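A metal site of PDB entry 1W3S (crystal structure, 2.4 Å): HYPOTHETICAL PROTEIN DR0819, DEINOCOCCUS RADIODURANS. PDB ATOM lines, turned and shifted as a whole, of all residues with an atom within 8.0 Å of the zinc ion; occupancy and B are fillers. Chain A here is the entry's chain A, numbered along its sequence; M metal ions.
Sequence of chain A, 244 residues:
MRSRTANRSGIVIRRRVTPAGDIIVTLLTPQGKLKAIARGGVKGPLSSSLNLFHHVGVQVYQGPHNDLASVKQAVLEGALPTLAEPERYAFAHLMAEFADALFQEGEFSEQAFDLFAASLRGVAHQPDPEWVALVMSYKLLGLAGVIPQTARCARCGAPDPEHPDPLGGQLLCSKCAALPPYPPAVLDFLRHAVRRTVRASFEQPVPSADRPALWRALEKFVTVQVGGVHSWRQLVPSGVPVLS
The side-chain sulfur (SG) of Cys 153 lies close to the backbone NH (N) of Arg 155, 3.4 Å away. The side-chain sulfur (SG) of Cys 176 sits close to the guanidinium group (NH1) of Arg 155, at 3.6 Å. The backbone NH (N) of Ala 158 lies close to the side-chain sulfur (SG) of Cys 156 (3.4 Å). The side-chain sulfur (SG) of Cys 173 lies close to the backbone NH (N) of Lys 175 (3.6 Å). The backbone NH of Cys 153 sits at hydrogen-bond distance from the backbone carbonyl oxygen of Ala 158 (2.9 Å).
Four residues have an atom within 4 Å of the zinc ion: Cys 153, Cys 156, Cys 173 and Cys 176.
The zinc ion is bound by the side-chain sulfur of Cys 176, the side-chain sulfur of Cys 156, the side-chain sulfur of Cys 173 and the side-chain sulfur of Cys 153.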
ATOM      1  N   ARG A 152       0.517 -14.257  -4.766  1.00  0.00           N
ATOM      2  CA  ARG A 152      -0.724 -13.851  -5.422  1.00  0.00           C
ATOM      3  C   ARG A 152      -1.740 -14.976  -5.426  1.00  0.00           C
ATOM      4  O   ARG A 152      -1.373 -16.156  -5.447  1.00  0.00           O
ATOM      5  CB  ARG A 152      -0.451 -13.384  -6.858  1.00  0.00           C
ATOM      6  CG  ARG A 152       0.095 -11.955  -6.919  1.00  0.00           C
ATOM      7  CD  ARG A 152       0.486 -11.486  -8.319  1.00  0.00           C
ATOM      8  NE  ARG A 152       0.281 -10.041  -8.496  1.00  0.00           N
ATOM      9  CZ  ARG A 152       0.985  -9.074  -7.899  1.00  0.00           C
ATOM     10  NH1 ARG A 152       1.960  -9.354  -7.028  1.00  0.00           N
ATOM     11  NH2 ARG A 152       0.704  -7.797  -8.155  1.00  0.00           N
ATOM     12  N   CYS A 153      -3.018 -14.595  -5.415  1.00  0.00           N
ATOM     13  CA  CYS A 153      -4.121 -15.549  -5.403  1.00  0.00           C
ATOM     14  C   CYS A 153      -4.218 -16.302  -6.717  1.00  0.00           C
ATOM     15  O   CYS A 153      -4.087 -15.735  -7.806  1.00  0.00           O
ATOM     16  CB  CYS A 153      -5.437 -14.833  -5.109  1.00  0.00           C
ATOM     17  SG  CYS A 153      -6.907 -15.843  -5.351  1.00  0.00           S
ATOM     18  N   ALA A 154      -4.459 -17.609  -6.609  1.00  0.00           N
ATOM     19  CA  ALA A 154      -4.438 -18.502  -7.753  1.00  0.00           C
ATOM     20  C   ALA A 154      -5.552 -18.206  -8.743  1.00  0.00           C
ATOM     21  O   ALA A 154      -5.413 -18.503  -9.940  1.00  0.00           O
ATOM     22  CB  ALA A 154      -4.525 -19.943  -7.285  1.00  0.00           C
ATOM     23  N   ARG A 155      -6.647 -17.625  -8.243  1.00  0.00           N
ATOM     24  CA  ARG A 155      -7.830 -17.349  -9.056  1.00  0.00           C
ATOM     25  C   ARG A 155      -7.840 -15.901  -9.542  1.00  0.00           C
ATOM     26  O   ARG A 155      -7.850 -15.646 -10.747  1.00  0.00           O
ATOM     27  CB  ARG A 155      -9.070 -17.643  -8.216  1.00  0.00           C
ATOM     28  CG  ARG A 155     -10.403 -17.564  -8.935  1.00  0.00           C
ATOM     29  CD  ARG A 155     -11.533 -18.077  -8.068  1.00  0.00           C
ATOM     30  NE  ARG A 155     -12.852 -17.993  -8.694  1.00  0.00           N
ATOM     31  CZ  ARG A 155     -13.737 -16.999  -8.526  1.00  0.00           C
ATOM     32  NH1 ARG A 155     -13.456 -15.931  -7.771  1.00  0.00           N
ATOM     33  NH2 ARG A 155     -14.904 -17.059  -9.152  1.00  0.00           N
ATOM     34  N   CYS A 156      -7.830 -14.947  -8.618  1.00  0.00           N
ATOM     35  CA  CYS A 156      -8.026 -13.543  -8.963  1.00  0.00           C
ATOM     36  C   CYS A 156      -6.740 -12.737  -9.053  1.00  0.00           C
ATOM     37  O   CYS A 156      -6.718 -11.684  -9.685  1.00  0.00           O
ATOM     38  CB  CYS A 156      -8.997 -12.883  -7.980  1.00  0.00           C
ATOM     39  SG  CYS A 156      -8.275 -12.402  -6.412  1.00  0.00           S
ATOM     40  N   GLY A 157      -5.670 -13.231  -8.419  1.00  0.00           N
ATOM     41  CA  GLY A 157      -4.356 -12.592  -8.483  1.00  0.00           C
ATOM     42  C   GLY A 157      -4.072 -11.623  -7.349  1.00  0.00           C
ATOM     43  O   GLY A 157      -3.058 -10.940  -7.365  1.00  0.00           O
ATOM     44  N   ALA A 158      -4.962 -11.565  -6.367  1.00  0.00           N
ATOM     45  CA  ALA A 158      -4.841 -10.641  -5.231  1.00  0.00           C
ATOM     46  C   ALA A 158      -3.640 -11.013  -4.357  1.00  0.00           C
ATOM     47  O   ALA A 158      -3.513 -12.171  -3.975  1.00  0.00           O
ATOM     48  CB  ALA A 158      -6.129 -10.662  -4.412  1.00  0.00           C
ATOM     49  N   PRO A 159      -2.778 -10.033  -4.033  1.00  0.00           N
ATOM     50  CA  PRO A 159      -1.597 -10.284  -3.194  1.00  0.00           C
ATOM     51  C   PRO A 159      -1.881 -10.900  -1.831  1.00  0.00           C
ATOM     52  O   PRO A 159      -2.928 -10.648  -1.247  1.00  0.00           O
ATOM     53  CB  PRO A 159      -0.993  -8.884  -2.995  1.00  0.00           C
ATOM     54  CG  PRO A 159      -1.511  -8.056  -4.107  1.00  0.00           C
ATOM     55  CD  PRO A 159      -2.842  -8.639  -4.476  1.00  0.00           C
ATOM     56  N   PRO A 161      -2.437 -14.046  -0.462  1.00  0.00           N
ATOM     57  CA  PRO A 161      -3.532 -14.969  -0.150  1.00  0.00           C
ATOM     58  C   PRO A 161      -3.186 -15.786   1.093  1.00  0.00           C
ATOM     59  O   PRO A 161      -2.017 -16.180   1.277  1.00  0.00           O
ATOM     60  CB  PRO A 161      -3.620 -15.856  -1.387  1.00  0.00           C
ATOM     61  CG  PRO A 161      -2.257 -15.757  -2.004  1.00  0.00           C
ATOM     62  CD  PRO A 161      -1.816 -14.351  -1.760  1.00  0.00           C
ATOM     63  N   LEU A 171      -2.625 -20.991  -3.188  1.00  0.00           N
ATOM     64  CA  LEU A 171      -3.234 -20.134  -2.170  1.00  0.00           C
ATOM     65  C   LEU A 171      -4.363 -19.285  -2.763  1.00  0.00           C
ATOM     66  O   LEU A 171      -4.193 -18.696  -3.829  1.00  0.00           O
ATOM     67  CB  LEU A 171      -2.178 -19.206  -1.591  1.00  0.00           C
ATOM     68  CG  LEU A 171      -1.065 -19.814  -0.729  1.00  0.00           C
ATOM     69  CD1 LEU A 171      -0.121 -18.689  -0.298  1.00  0.00           C
ATOM     70  CD2 LEU A 171      -1.614 -20.573   0.487  1.00  0.00           C
ATOM     71  N   LEU A 172      -5.499 -19.234  -2.072  1.00  0.00           N
ATOM     72  CA  LEU A 172      -6.621 -18.363  -2.460  1.00  0.00           C
ATOM     73  C   LEU A 172      -6.798 -17.225  -1.460  1.00  0.00           C
ATOM     74  O   LEU A 172      -6.505 -17.386  -0.294  1.00  0.00           O
ATOM     75  CB  LEU A 172      -7.913 -19.183  -2.535  1.00  0.00           C
ATOM     76  CG  LEU A 172      -7.958 -20.237  -3.640  1.00  0.00           C
ATOM     77  CD1 LEU A 172      -9.144 -21.184  -3.449  1.00  0.00           C
ATOM     78  CD2 LEU A 172      -7.995 -19.583  -5.039  1.00  0.00           C
ATOM     79  N   CYS A 173      -7.260 -16.073  -1.932  1.00  0.00           N
ATOM     80  CA  CYS A 173      -7.605 -14.970  -1.039  1.00  0.00           C
ATOM     81  C   CYS A 173      -8.959 -15.237  -0.374  1.00  0.00           C
ATOM     82  O   CYS A 173      -9.695 -16.123  -0.795  1.00  0.00           O
ATOM     83  CB  CYS A 173      -7.640 -13.632  -1.779  1.00  0.00           C
ATOM     84  SG  CYS A 173      -9.082 -13.466  -2.863  1.00  0.00           S
ATOM     85  N   SER A 174      -9.275 -14.454   0.652  1.00  0.00           N
ATOM     86  CA  SER A 174     -10.503 -14.651   1.432  1.00  0.00           C
ATOM     87  C   SER A 174     -11.760 -14.626   0.576  1.00  0.00           C
ATOM     88  O   SER A 174     -12.729 -15.304   0.895  1.00  0.00           O
ATOM     89  CB  SER A 174     -10.613 -13.583   2.524  1.00  0.00           C
ATOM     90  OG  SER A 174     -10.526 -12.287   1.992  1.00  0.00           O
ATOM     91  N   LYS A 175     -11.732 -13.872  -0.521  1.00  0.00           N
ATOM     92  CA  LYS A 175     -12.904 -13.649  -1.356  1.00  0.00           C
ATOM     93  C   LYS A 175     -13.096 -14.750  -2.407  1.00  0.00           C
ATOM     94  O   LYS A 175     -14.192 -14.920  -2.926  1.00  0.00           O
ATOM     95  CB  LYS A 175     -12.792 -12.291  -2.047  1.00  0.00           C
ATOM     96  CG  LYS A 175     -12.282 -11.137  -1.167  1.00  0.00           C
ATOM     97  CD  LYS A 175     -13.369 -10.156  -0.777  1.00  0.00           C
ATOM     98  CE  LYS A 175     -12.754  -8.892  -0.168  1.00  0.00           C
ATOM     99  NZ  LYS A 175     -13.763  -7.768   0.009  1.00  0.00           N
ATOM    100  N   CYS A 176     -12.032 -15.461  -2.745  1.00  0.00           N
ATOM    101  CA  CYS A 176     -12.134 -16.659  -3.593  1.00  0.00           C
ATOM    102  C   CYS A 176     -12.299 -17.935  -2.770  1.00  0.00           C
ATOM    103  O   CYS A 176     -12.760 -18.948  -3.294  1.00  0.00           O
ATOM    104  CB  CYS A 176     -10.909 -16.792  -4.478  1.00  0.00           C
ATOM    105  SG  CYS A 176     -10.662 -15.435  -5.620  1.00  0.00           S
ATOM    106  N   ALA A 177     -11.916 -17.880  -1.486  1.00  0.00           N
ATOM    107  CA  ALA A 177     -11.813 -19.087  -0.652  1.00  0.00           C
ATOM    108  C   ALA A 177     -13.104 -19.444   0.075  1.00  0.00           C
ATOM    109  O   ALA A 177     -13.785 -18.571   0.608  1.00  0.00           O
ATOM    110  CB  ALA A 177     -10.695 -18.931   0.362  1.00  0.00           C
HETATM  111 ZN    ZN M   1      -8.845 -14.201  -5.196  1.00  0.00          ZN
